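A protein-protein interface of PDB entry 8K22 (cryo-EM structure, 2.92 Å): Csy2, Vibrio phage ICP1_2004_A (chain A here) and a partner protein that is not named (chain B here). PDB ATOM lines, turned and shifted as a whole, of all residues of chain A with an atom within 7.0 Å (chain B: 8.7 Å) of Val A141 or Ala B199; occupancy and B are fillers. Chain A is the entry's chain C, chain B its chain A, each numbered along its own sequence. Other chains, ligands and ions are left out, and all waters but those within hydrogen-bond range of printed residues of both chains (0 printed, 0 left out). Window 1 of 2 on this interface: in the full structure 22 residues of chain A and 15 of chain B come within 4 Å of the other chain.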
ATOM      1  N   MET A   1     -10.793  11.033  10.809  1.00  0.00           N
ATOM      2  CA  MET A   1      -9.481  10.810  11.399  1.00  0.00           C
ATOM      3  C   MET A   1      -8.844   9.650  10.630  1.00  0.00           C
ATOM      4  O   MET A   1      -9.400   8.554  10.570  1.00  0.00           O
ATOM      5  CB  MET A   1      -9.619  10.530  12.901  1.00  0.00           C
ATOM      6  CG  MET A   1      -8.376  10.783  13.755  1.00  0.00           C
ATOM      7  SD  MET A   1      -6.965   9.728  13.419  1.00  0.00           S
ATOM      8  CE  MET A   1      -7.766   8.129  13.541  1.00  0.00           C
ATOM      9  N   ARG A   2      -7.669   9.903  10.048  1.00  0.00           N
ATOM     10  CA  ARG A   2      -7.092   9.062   9.005  1.00  0.00           C
ATOM     11  C   ARG A   2      -5.736   8.543   9.467  1.00  0.00           C
ATOM     12  O   ARG A   2      -5.005   9.253  10.159  1.00  0.00           O
ATOM     13  CB  ARG A   2      -6.952   9.873   7.712  1.00  0.00           C
ATOM     14  CG  ARG A   2      -8.210  10.681   7.409  1.00  0.00           C
ATOM     15  CD  ARG A   2      -8.285  11.318   6.043  1.00  0.00           C
ATOM     16  NE  ARG A   2      -8.482  10.379   4.949  1.00  0.00           N
ATOM     17  CZ  ARG A   2      -8.377  10.716   3.673  1.00  0.00           C
ATOM     18  NH1 ARG A   2      -8.066  11.947   3.311  1.00  0.00           N
ATOM     19  NH2 ARG A   2      -8.614   9.804   2.738  1.00  0.00           N
ATOM     20  N   LYS A   3      -5.403   7.304   9.101  1.00  0.00           N
ATOM     21  CA  LYS A   3      -4.115   6.698   9.437  1.00  0.00           C
ATOM     22  C   LYS A   3      -3.464   6.132   8.181  1.00  0.00           C
ATOM     23  O   LYS A   3      -4.141   5.525   7.345  1.00  0.00           O
ATOM     24  CB  LYS A   3      -4.267   5.586  10.481  1.00  0.00           C
ATOM     25  CG  LYS A   3      -5.356   5.804  11.516  1.00  0.00           C
ATOM     26  CD  LYS A   3      -5.604   4.550  12.318  1.00  0.00           C
ATOM     27  CE  LYS A   3      -6.995   4.565  12.899  1.00  0.00           C
ATOM     28  NZ  LYS A   3      -8.047   4.545  11.862  1.00  0.00           N
ATOM     29  N   PHE A   4      -2.145   6.298   8.067  1.00  0.00           N
ATOM     30  CA  PHE A   4      -1.396   5.900   6.888  1.00  0.00           C
ATOM     31  C   PHE A   4      -0.119   5.190   7.299  1.00  0.00           C
ATOM     32  O   PHE A   4       0.470   5.494   8.341  1.00  0.00           O
ATOM     33  CB  PHE A   4      -1.002   7.106   6.035  1.00  0.00           C
ATOM     34  CG  PHE A   4      -2.156   7.904   5.522  1.00  0.00           C
ATOM     35  CD1 PHE A   4      -2.723   8.916   6.279  1.00  0.00           C
ATOM     36  CD2 PHE A   4      -2.655   7.660   4.261  1.00  0.00           C
ATOM     37  CE1 PHE A   4      -3.777   9.651   5.787  1.00  0.00           C
ATOM     38  CE2 PHE A   4      -3.696   8.392   3.767  1.00  0.00           C
ATOM     39  CZ  PHE A   4      -4.266   9.387   4.528  1.00  0.00           C
ATOM     40  N   TRP A 106      -6.183   0.932  12.012  1.00  0.00           N
ATOM     41  CA  TRP A 106      -5.450   0.049  12.898  1.00  0.00           C
ATOM     42  C   TRP A 106      -5.780   0.416  14.334  1.00  0.00           C
ATOM     43  O   TRP A 106      -6.107   1.565  14.637  1.00  0.00           O
ATOM     44  CB  TRP A 106      -3.944   0.156  12.627  1.00  0.00           C
ATOM     45  CG  TRP A 106      -3.084  -0.904  13.241  1.00  0.00           C
ATOM     46  CD1 TRP A 106      -2.053  -0.697  14.104  1.00  0.00           C
ATOM     47  CD2 TRP A 106      -3.172  -2.323  13.056  1.00  0.00           C
ATOM     48  NE1 TRP A 106      -1.485  -1.890  14.462  1.00  0.00           N
ATOM     49  CE2 TRP A 106      -2.155  -2.905  13.835  1.00  0.00           C
ATOM     50  CE3 TRP A 106      -4.005  -3.157  12.307  1.00  0.00           C
ATOM     51  CZ2 TRP A 106      -1.951  -4.278  13.891  1.00  0.00           C
ATOM     52  CZ3 TRP A 106      -3.805  -4.520  12.371  1.00  0.00           C
ATOM     53  CH2 TRP A 106      -2.784  -5.068  13.150  1.00  0.00           C
ATOM     54  N   GLU A 107      -5.708  -0.577  15.215  1.00  0.00           N
ATOM     55  CA  GLU A 107      -6.120  -0.383  16.595  1.00  0.00           C
ATOM     56  C   GLU A 107      -5.033  -0.820  17.564  1.00  0.00           C
ATOM     57  O   GLU A 107      -5.225  -0.766  18.783  1.00  0.00           O
ATOM     58  CB  GLU A 107      -7.416  -1.151  16.890  1.00  0.00           C
ATOM     59  CG  GLU A 107      -8.752  -0.738  16.183  1.00  0.00           C
ATOM     60  CD  GLU A 107      -8.945   0.731  15.757  1.00  0.00           C
ATOM     61  OE1 GLU A 107      -8.485   1.688  16.422  1.00  0.00           O
ATOM     62  OE2 GLU A 107      -9.587   0.927  14.705  1.00  0.00           O
ATOM     63  N   VAL A 139       4.634   4.855  10.118  1.00  0.00           N
ATOM     64  CA  VAL A 139       3.228   5.181  10.287  1.00  0.00           C
ATOM     65  C   VAL A 139       3.103   6.676  10.530  1.00  0.00           C
ATOM     66  O   VAL A 139       3.814   7.237  11.370  1.00  0.00           O
ATOM     67  CB  VAL A 139       2.615   4.387  11.448  1.00  0.00           C
ATOM     68  CG1 VAL A 139       1.142   4.644  11.521  1.00  0.00           C
ATOM     69  CG2 VAL A 139       2.890   2.915  11.267  1.00  0.00           C
ATOM     70  N   LYS A 140       2.212   7.323   9.786  1.00  0.00           N
ATOM     71  CA  LYS A 140       1.894   8.719  10.030  1.00  0.00           C
ATOM     72  C   LYS A 140       0.386   8.894   9.961  1.00  0.00           C
ATOM     73  O   LYS A 140      -0.289   8.231   9.172  1.00  0.00           O
ATOM     74  CB  LYS A 140       2.612   9.636   9.037  1.00  0.00           C
ATOM     75  CG  LYS A 140       3.994  10.049   9.515  1.00  0.00           C
ATOM     76  CD  LYS A 140       4.683  10.983   8.543  1.00  0.00           C
ATOM     77  CE  LYS A 140       3.973  12.324   8.464  1.00  0.00           C
ATOM     78  NZ  LYS A 140       3.545  12.813   9.804  1.00  0.00           N
ATOM     79  N   VAL A 141      -0.142   9.788  10.789  1.00  0.00           N
ATOM     80  CA  VAL A 141      -1.592   9.946  10.883  1.00  0.00           C
ATOM     81  C   VAL A 141      -2.091  11.295  10.378  1.00  0.00           C
ATOM     82  O   VAL A 141      -1.404  12.304  10.520  1.00  0.00           O
ATOM     83  CB  VAL A 141      -2.006   9.660  12.350  1.00  0.00           C
ATOM     84  CG1 VAL A 141      -3.164  10.513  12.849  1.00  0.00           C
ATOM     85  CG2 VAL A 141      -2.264   8.178  12.539  1.00  0.00           C
ATOM     86  N   ALA A 142      -3.256  11.308   9.740  1.00  0.00           N
ATOM     87  CA  ALA A 142      -3.842  12.558   9.282  1.00  0.00           C
ATOM     88  C   ALA A 142      -5.038  12.937  10.134  1.00  0.00           C
ATOM     89  O   ALA A 142      -6.178  12.693   9.744  1.00  0.00           O
ATOM     90  CB  ALA A 142      -4.271  12.429   7.845  1.00  0.00           C
ATOM     91  N   LYS A 143      -4.792  13.531  11.294  1.00  0.00           N
ATOM     92  CA  LYS A 143      -5.888  13.980  12.141  1.00  0.00           C
ATOM     93  C   LYS A 143      -6.676  15.070  11.431  1.00  0.00           C
ATOM     94  O   LYS A 143      -7.889  14.954  11.261  1.00  0.00           O
ATOM     95  CB  LYS A 143      -5.360  14.499  13.478  1.00  0.00           C
ATOM     96  N   ASP A 144      -5.990  16.128  11.010  1.00  0.00           N
ATOM     97  CA  ASP A 144      -6.656  17.205  10.283  1.00  0.00           C
ATOM     98  C   ASP A 144      -6.145  17.265   8.853  1.00  0.00           C
ATOM     99  O   ASP A 144      -5.542  16.310   8.368  1.00  0.00           O
ATOM    100  CB  ASP A 144      -6.438  18.550  10.981  1.00  0.00           C
ATOM    101  CG  ASP A 144      -5.077  18.655  11.635  1.00  0.00           C
ATOM    102  OD1 ASP A 144      -4.940  18.244  12.806  1.00  0.00           O
ATOM    103  OD2 ASP A 144      -4.143  19.152  10.979  1.00  0.00           O
ATOM    104  N   GLU A 146      -3.983  19.634   7.746  1.00  0.00           N
ATOM    105  CA  GLU A 146      -2.563  19.968   7.783  1.00  0.00           C
ATOM    106  C   GLU A 146      -1.788  18.701   8.080  1.00  0.00           C
ATOM    107  O   GLU A 146      -0.667  18.526   7.605  1.00  0.00           O
ATOM    108  CB  GLU A 146      -2.276  21.040   8.833  1.00  0.00           C
ATOM    109  N   GLU A 147      -2.388  17.801   8.853  1.00  0.00           N
ATOM    110  CA  GLU A 147      -1.750  16.526   9.141  1.00  0.00           C
ATOM    111  C   GLU A 147      -1.846  15.625   7.923  1.00  0.00           C
ATOM    112  O   GLU A 147      -1.011  14.745   7.736  1.00  0.00           O
ATOM    113  CB  GLU A 147      -2.417  15.868  10.339  1.00  0.00           C
ATOM    114  CG  GLU A 147      -1.773  16.199  11.671  1.00  0.00           C
ATOM    115  CD  GLU A 147      -1.157  14.983  12.329  1.00  0.00           C
ATOM    116  OE1 GLU A 147       0.048  14.734  12.113  1.00  0.00           O
ATOM    117  OE2 GLU A 147      -1.878  14.269  13.057  1.00  0.00           O
ATOM    118  N   LEU A 148      -2.858  15.838   7.088  1.00  0.00           N
ATOM    119  CA  LEU A 148      -2.977  15.071   5.854  1.00  0.00           C
ATOM    120  C   LEU A 148      -1.850  15.483   4.938  1.00  0.00           C
ATOM    121  O   LEU A 148      -1.259  14.649   4.255  1.00  0.00           O
ATOM    122  CB  LEU A 148      -4.332  15.334   5.195  1.00  0.00           C
ATOM    123  CG  LEU A 148      -4.673  14.639   3.881  1.00  0.00           C
ATOM    124  CD1 LEU A 148      -4.909  13.158   4.111  1.00  0.00           C
ATOM    125  CD2 LEU A 148      -5.880  15.285   3.221  1.00  0.00           C
ATOM    126  N   SER A 150       0.970  16.581   5.990  1.00  0.00           N
ATOM    127  CA  SER A 150       2.210  16.094   6.572  1.00  0.00           C
ATOM    128  C   SER A 150       2.479  14.719   5.999  1.00  0.00           C
ATOM    129  O   SER A 150       3.589  14.440   5.557  1.00  0.00           O
ATOM    130  CB  SER A 150       2.115  16.034   8.095  1.00  0.00           C
ATOM    131  OG  SER A 150       3.400  15.912   8.676  1.00  0.00           O
ATOM    132  N   VAL A 151       1.460  13.865   5.986  1.00  0.00           N
ATOM    133  CA  VAL A 151       1.603  12.536   5.401  1.00  0.00           C
ATOM    134  C   VAL A 151       1.935  12.662   3.924  1.00  0.00           C
ATOM    135  O   VAL A 151       2.800  11.952   3.406  1.00  0.00           O
ATOM    136  CB  VAL A 151       0.303  11.732   5.567  1.00  0.00           C
ATOM    137  CG1 VAL A 151       0.431  10.370   4.922  1.00  0.00           C
ATOM    138  CG2 VAL A 151      -0.049  11.592   7.036  1.00  0.00           C
ATOM    139  N   VAL B 192       3.841   9.271  24.651  1.00  0.00           N
ATOM    140  CA  VAL B 192       3.499   8.220  23.696  1.00  0.00           C
ATOM    141  C   VAL B 192       3.885   8.719  22.308  1.00  0.00           C
ATOM    142  O   VAL B 192       3.315   9.693  21.804  1.00  0.00           O
ATOM    143  CB  VAL B 192       2.015   7.844  23.768  1.00  0.00           C
ATOM    144  CG1 VAL B 192       1.735   6.616  22.917  1.00  0.00           C
ATOM    145  CG2 VAL B 192       1.608   7.589  25.211  1.00  0.00           C
ATOM    146  N   GLU B 193       4.860   8.054  21.688  1.00  0.00           N
ATOM    147  CA  GLU B 193       5.304   8.359  20.334  1.00  0.00           C
ATOM    148  C   GLU B 193       4.443   7.717  19.262  1.00  0.00           C
ATOM    149  O   GLU B 193       4.573   8.077  18.086  1.00  0.00           O
ATOM    150  CB  GLU B 193       6.750   7.891  20.125  1.00  0.00           C
ATOM    151  CG  GLU B 193       7.823   8.656  20.861  1.00  0.00           C
ATOM    152  CD  GLU B 193       7.447  10.086  21.138  1.00  0.00           C
ATOM    153  OE1 GLU B 193       7.383  10.899  20.189  1.00  0.00           O
ATOM    154  OE2 GLU B 193       7.222  10.405  22.309  1.00  0.00           O
ATOM    155  N   ASP B 194       3.577   6.790  19.634  1.00  0.00           N
ATOM    156  CA  ASP B 194       2.939   5.923  18.656  1.00  0.00           C
ATOM    157  C   ASP B 194       1.851   6.675  17.897  1.00  0.00           C
ATOM    158  O   ASP B 194       0.953   7.249  18.521  1.00  0.00           O
ATOM    159  CB  ASP B 194       2.354   4.709  19.357  1.00  0.00           C
ATOM    160  CG  ASP B 194       2.236   3.520  18.448  1.00  0.00           C
ATOM    161  OD1 ASP B 194       3.223   2.771  18.336  1.00  0.00           O
ATOM    162  OD2 ASP B 194       1.162   3.342  17.838  1.00  0.00           O
ATOM    163  N   PRO B 195       1.897   6.694  16.562  1.00  0.00           N
ATOM    164  CA  PRO B 195       0.893   7.465  15.810  1.00  0.00           C
ATOM    165  C   PRO B 195      -0.490   6.846  15.829  1.00  0.00           C
ATOM    166  O   PRO B 195      -1.478   7.585  15.876  1.00  0.00           O
ATOM    167  CB  PRO B 195       1.478   7.507  14.391  1.00  0.00           C
ATOM    168  CG  PRO B 195       2.925   7.127  14.552  1.00  0.00           C
ATOM    169  CD  PRO B 195       2.953   6.169  15.687  1.00  0.00           C
ATOM    170  N   ILE B 196      -0.595   5.516  15.793  1.00  0.00           N
ATOM    171  CA  ILE B 196      -1.903   4.867  15.851  1.00  0.00           C
ATOM    172  C   ILE B 196      -2.520   5.041  17.233  1.00  0.00           C
ATOM    173  O   ILE B 196      -3.728   5.289  17.368  1.00  0.00           O
ATOM    174  CB  ILE B 196      -1.778   3.382  15.474  1.00  0.00           C
ATOM    175  CG1 ILE B 196      -1.171   3.232  14.079  1.00  0.00           C
ATOM    176  CG2 ILE B 196      -3.139   2.724  15.483  1.00  0.00           C
ATOM    177  CD1 ILE B 196      -2.080   3.677  12.959  1.00  0.00           C
ATOM    178  N   TYR B 197      -1.697   4.917  18.279  1.00  0.00           N
ATOM    179  CA  TYR B 197      -2.169   5.150  19.638  1.00  0.00           C
ATOM    180  C   TYR B 197      -2.606   6.596  19.828  1.00  0.00           C
ATOM    181  O   TYR B 197      -3.680   6.852  20.376  1.00  0.00           O
ATOM    182  CB  TYR B 197      -1.081   4.769  20.638  1.00  0.00           C
ATOM    183  CG  TYR B 197      -0.955   3.277  20.877  1.00  0.00           C
ATOM    184  CD1 TYR B 197      -1.975   2.407  20.513  1.00  0.00           C
ATOM    185  CD2 TYR B 197       0.188   2.741  21.458  1.00  0.00           C
ATOM    186  CE1 TYR B 197      -1.864   1.044  20.733  1.00  0.00           C
ATOM    187  CE2 TYR B 197       0.307   1.380  21.681  1.00  0.00           C
ATOM    188  CZ  TYR B 197      -0.722   0.539  21.320  1.00  0.00           C
ATOM    189  OH  TYR B 197      -0.604  -0.812  21.537  1.00  0.00           O
ATOM    190  N   ARG B 198      -1.821   7.552  19.316  1.00  0.00           N
ATOM    191  CA  ARG B 198      -2.218   8.958  19.339  1.00  0.00           C
ATOM    192  C   ARG B 198      -3.459   9.224  18.497  1.00  0.00           C
ATOM    193  O   ARG B 198      -4.206  10.167  18.780  1.00  0.00           O
ATOM    194  CB  ARG B 198      -1.075   9.840  18.840  1.00  0.00           C
ATOM    195  CG  ARG B 198       0.000  10.126  19.869  1.00  0.00           C
ATOM    196  CD  ARG B 198       1.075  11.006  19.271  1.00  0.00           C
ATOM    197  NE  ARG B 198       0.558  12.327  18.941  1.00  0.00           N
ATOM    198  CZ  ARG B 198       1.158  13.183  18.126  1.00  0.00           C
ATOM    199  NH1 ARG B 198       2.286  12.875  17.510  1.00  0.00           N
ATOM    200  NH2 ARG B 198       0.605  14.374  17.915  1.00  0.00           N
ATOM    201  N   ALA B 199      -3.695   8.405  17.478  1.00  0.00           N
ATOM    202  CA  ALA B 199      -4.851   8.555  16.613  1.00  0.00           C
ATOM    203  C   ALA B 199      -6.130   8.064  17.273  1.00  0.00           C
ATOM    204  O   ALA B 199      -7.194   8.662  17.089  1.00  0.00           O
ATOM    205  CB  ALA B 199      -4.596   7.787  15.324  1.00  0.00           C
ATOM    206  N   THR B 200      -6.050   6.977  18.040  1.00  0.00           N
ATOM    207  CA  THR B 200      -7.241   6.247  18.456  1.00  0.00           C
ATOM    208  C   THR B 200      -7.549   6.285  19.946  1.00  0.00           C
ATOM    209  O   THR B 200      -8.722   6.182  20.309  1.00  0.00           O
ATOM    210  CB  THR B 200      -7.128   4.781  18.033  1.00  0.00           C
ATOM    211  OG1 THR B 200      -6.006   4.191  18.694  1.00  0.00           O
ATOM    212  CG2 THR B 200      -6.929   4.679  16.549  1.00  0.00           C
ATOM    213  N   LYS B 201      -6.551   6.407  20.818  1.00  0.00           N
ATOM    214  CA  LYS B 201      -6.789   6.183  22.240  1.00  0.00           C
ATOM    215  C   LYS B 201      -7.501   7.372  22.879  1.00  0.00           C
ATOM    216  O   LYS B 201      -7.070   8.521  22.740  1.00  0.00           O
ATOM    217  CB  LYS B 201      -5.476   5.892  22.962  1.00  0.00           C
ATOM    218  CG  LYS B 201      -4.741   4.644  22.476  1.00  0.00           C
ATOM    219  CD  LYS B 201      -5.578   3.393  22.620  1.00  0.00           C
ATOM    220  CE  LYS B 201      -5.511   2.504  21.401  1.00  0.00           C
ATOM    221  NZ  LYS B 201      -6.241   1.228  21.612  1.00  0.00           N
ATOM    222  N   THR B 202      -8.605   7.090  23.568  1.00  0.00           N
ATOM    223  CA  THR B 202      -9.486   8.106  24.136  1.00  0.00           C
ATOM    224  C   THR B 202      -9.813   7.887  25.606  1.00  0.00           C
ATOM    225  O   THR B 202      -9.804   8.847  26.383  1.00  0.00           O
ATOM    226  CB  THR B 202     -10.784   8.140  23.310  1.00  0.00           C
ATOM    227  OG1 THR B 202     -10.470   8.406  21.938  1.00  0.00           O
ATOM    228  CG2 THR B 202     -11.755   9.193  23.824  1.00  0.00           C
ATOM    229  N   GLU B 206      -7.827   2.724  28.563  1.00  0.00           N
ATOM    230  CA  GLU B 206      -7.540   2.284  27.208  1.00  0.00           C
ATOM    231  C   GLU B 206      -6.425   3.124  26.594  1.00  0.00           C
ATOM    232  O   GLU B 206      -5.690   2.635  25.732  1.00  0.00           O
ATOM    233  CB  GLU B 206      -8.859   2.279  26.422  1.00  0.00           C
ATOM    234  CG  GLU B 206      -8.871   2.313  24.900  1.00  0.00           C
ATOM    235  CD  GLU B 206      -8.771   3.693  24.307  1.00  0.00           C
ATOM    236  OE1 GLU B 206      -8.771   4.686  25.063  1.00  0.00           O
ATOM    237  OE2 GLU B 206      -8.801   3.775  23.065  1.00  0.00           O
ATOM    238  N   ASP B 843     -13.085  17.644  19.527  1.00  0.00           N
ATOM    239  CA  ASP B 843     -12.586  16.288  19.671  1.00  0.00           C
ATOM    240  C   ASP B 843     -11.508  16.274  20.730  1.00  0.00           C
ATOM    241  O   ASP B 843     -11.174  17.313  21.297  1.00  0.00           O
ATOM    242  CB  ASP B 843     -12.015  15.786  18.344  1.00  0.00           C
ATOM    243  CG  ASP B 843     -12.230  14.301  18.140  1.00  0.00           C
ATOM    244  OD1 ASP B 843     -13.347  13.912  17.743  1.00  0.00           O
ATOM    245  OD2 ASP B 843     -11.281  13.526  18.384  1.00  0.00           O
ATOM    246  N   ILE B 844     -10.960  15.099  21.006  1.00  0.00           N
ATOM    247  CA  ILE B 844      -9.879  15.003  21.969  1.00  0.00           C
ATOM    248  C   ILE B 844      -8.548  14.865  21.244  1.00  0.00           C
ATOM    249  O   ILE B 844      -7.534  15.334  21.754  1.00  0.00           O
ATOM    250  CB  ILE B 844     -10.102  13.847  22.974  1.00  0.00           C
ATOM    251  CG1 ILE B 844     -10.142  12.488  22.276  1.00  0.00           C
ATOM    252  CG2 ILE B 844     -11.396  14.049  23.745  1.00  0.00           C
ATOM    253  CD1 ILE B 844      -8.956  11.612  22.602  1.00  0.00           C
ATOM    254  N   ALA B 845      -8.549  14.255  20.057  1.00  0.00           N
ATOM    255  CA  ALA B 845      -7.318  14.032  19.286  1.00  0.00           C
ATOM    256  C   ALA B 845      -6.080  13.781  20.135  1.00  0.00           C
ATOM    257  O   ALA B 845      -5.979  12.745  20.795  1.00  0.00           O
ATOM    258  CB  ALA B 845      -7.077  15.187  18.320  1.00  0.00           C
ATOM    259  N   ASP B 846      -5.139  14.718  20.110  1.00  0.00           N
ATOM    260  CA  ASP B 846      -3.929  14.599  20.916  1.00  0.00           C
ATOM    261  C   ASP B 846      -3.421  16.010  21.103  1.00  0.00           C
ATOM    262  O   ASP B 846      -2.740  16.317  22.083  1.00  0.00           O
ATOM    263  CB  ASP B 846      -2.878  13.760  20.197  1.00  0.00           C
ATOM    264  CG  ASP B 846      -1.810  13.258  21.131  1.00  0.00           C
ATOM    265  OD1 ASP B 846      -2.046  12.242  21.812  1.00  0.00           O
ATOM    266  OD2 ASP B 846      -0.736  13.884  21.186  1.00  0.00           O
ATOM    267  N   TRP B 854      -5.481  11.800  27.515  1.00  0.00           N
ATOM    268  CA  TRP B 854      -4.134  12.168  27.215  1.00  0.00           C
ATOM    269  C   TRP B 854      -3.620  13.108  28.275  1.00  0.00           C
ATOM    270  O   TRP B 854      -2.443  13.371  28.317  1.00  0.00           O
ATOM    271  CB  TRP B 854      -4.055  12.827  25.852  1.00  0.00           C
ATOM    272  CG  TRP B 854      -4.368  11.916  24.762  1.00  0.00           C
ATOM    273  CD1 TRP B 854      -5.488  11.914  24.000  1.00  0.00           C
ATOM    274  CD2 TRP B 854      -3.557  10.843  24.296  1.00  0.00           C
ATOM    275  NE1 TRP B 854      -5.425  10.905  23.078  1.00  0.00           N
ATOM    276  CE2 TRP B 854      -4.244  10.234  23.242  1.00  0.00           C
ATOM    277  CE3 TRP B 854      -2.308  10.345  24.660  1.00  0.00           C
ATOM    278  CZ2 TRP B 854      -3.732   9.152  22.560  1.00  0.00           C
ATOM    279  CZ3 TRP B 854      -1.803   9.272  23.983  1.00  0.00           C
ATOM    280  CH2 TRP B 854      -2.510   8.684  22.945  1.00  0.00           C
ATOM    281  N   ASN B 859       1.620  13.765  26.279  1.00  0.00           N
ATOM    282  CA  ASN B 859       1.341  14.150  24.897  1.00  0.00           C
ATOM    283  C   ASN B 859       0.784  15.564  24.679  1.00  0.00           C
ATOM    284  O   ASN B 859       1.245  16.215  23.726  1.00  0.00           O
ATOM    285  CB  ASN B 859       0.421  13.097  24.273  1.00  0.00           C
ATOM    286  CG  ASN B 859       1.112  11.764  24.092  1.00  0.00           C
ATOM    287  OD1 ASN B 859       1.788  11.273  24.996  1.00  0.00           O
ATOM    288  ND2 ASN B 859       0.950  11.170  22.921  1.00  0.00           N
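Of the printed residues of chain B, Glu A107 touches Thr B200 and Lys B201.
Val A141 touches two residues of chain B.
No residue of chain B comes within 4 Å of Ala A142.
Glu A146 touches none of the printed residues of chain B.
Of the printed residues of chain A, Pro B195 touches Val A139 (3.3 Å) and Val A141 (3.5 Å).
Of chain A, only Met A1 and Val A141 come within 4 Å of Ala B199.
Of the printed residues of chain A, Thr B200 touches Lys A3 (3.7 Å), Trp A106 (3.7 Å) and Glu A107 (3.4 Å).
Asp B843 touches none of the printed residues of chain A.
The nearest printed residue of chain B that does not touch Lys A3 is Ala B199 (4.4 Å).
CD1 of Ile B196 touches CD of Lys A3, at 3.7 Å.
Lys A3 touches Thr B200 (CE to CG2, 3.7 Å).
Trp A106 touches Ile B196 (O to CG2, 3.3 Å).
Thr B200 touches Trp A106 (CG2 to O, 3.7 Å).
CG2 of Thr B200 touches OE1 of Glu A107, at 3.4 Å.
Glu A107 touches Lys B201 (O to NZ, 3.6 Å).
CG of Pro B195 touches O of Val A139 (3.3 Å).
Ile B196 touches Val A139 (CD1 to CG1, 3.7 Å).
Pro B195 touches Val A141 (O to CG2, 3.5 Å).
Val A141 touches Ala B199.
Of the 17 printed residues of chain A, 6 touch a printed residue of chain B.
Hydrophobic or aromatic side chains of chain B within 4 Å of the printed part of chain A: Pro B195, Ile B196 and Ala B199.
Along chain B the printed residues that touch a printed residue of chain A span positions 195 to 201.
Among the printed residues, 11 pairs touch across the chains.
Among the printed residues, no Asp or Glu carboxylate lies within 4 Å of a Lys or Arg side-chain nitrogen of the other chain.
The side-chain carboxylate (OD2) of Asp B194 sits close to the backbone NH (N) of Ile B196.
OG1 of Thr B200 lies within hydrogen-bond range of O of Ile B196 (2.9 Å).
O of Thr B200 is in hydrogen-bond range of OG1 of Thr B202, 3.3 Å away.
NZ of Lys B201 is in salt-bridge range of OE2 of Glu B206.
The backbone carbonyl oxygen (O) of Lys B201 is in hydrogen-bond range of the indole nitrogen (NE1) of Trp B854 (2.9 Å).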
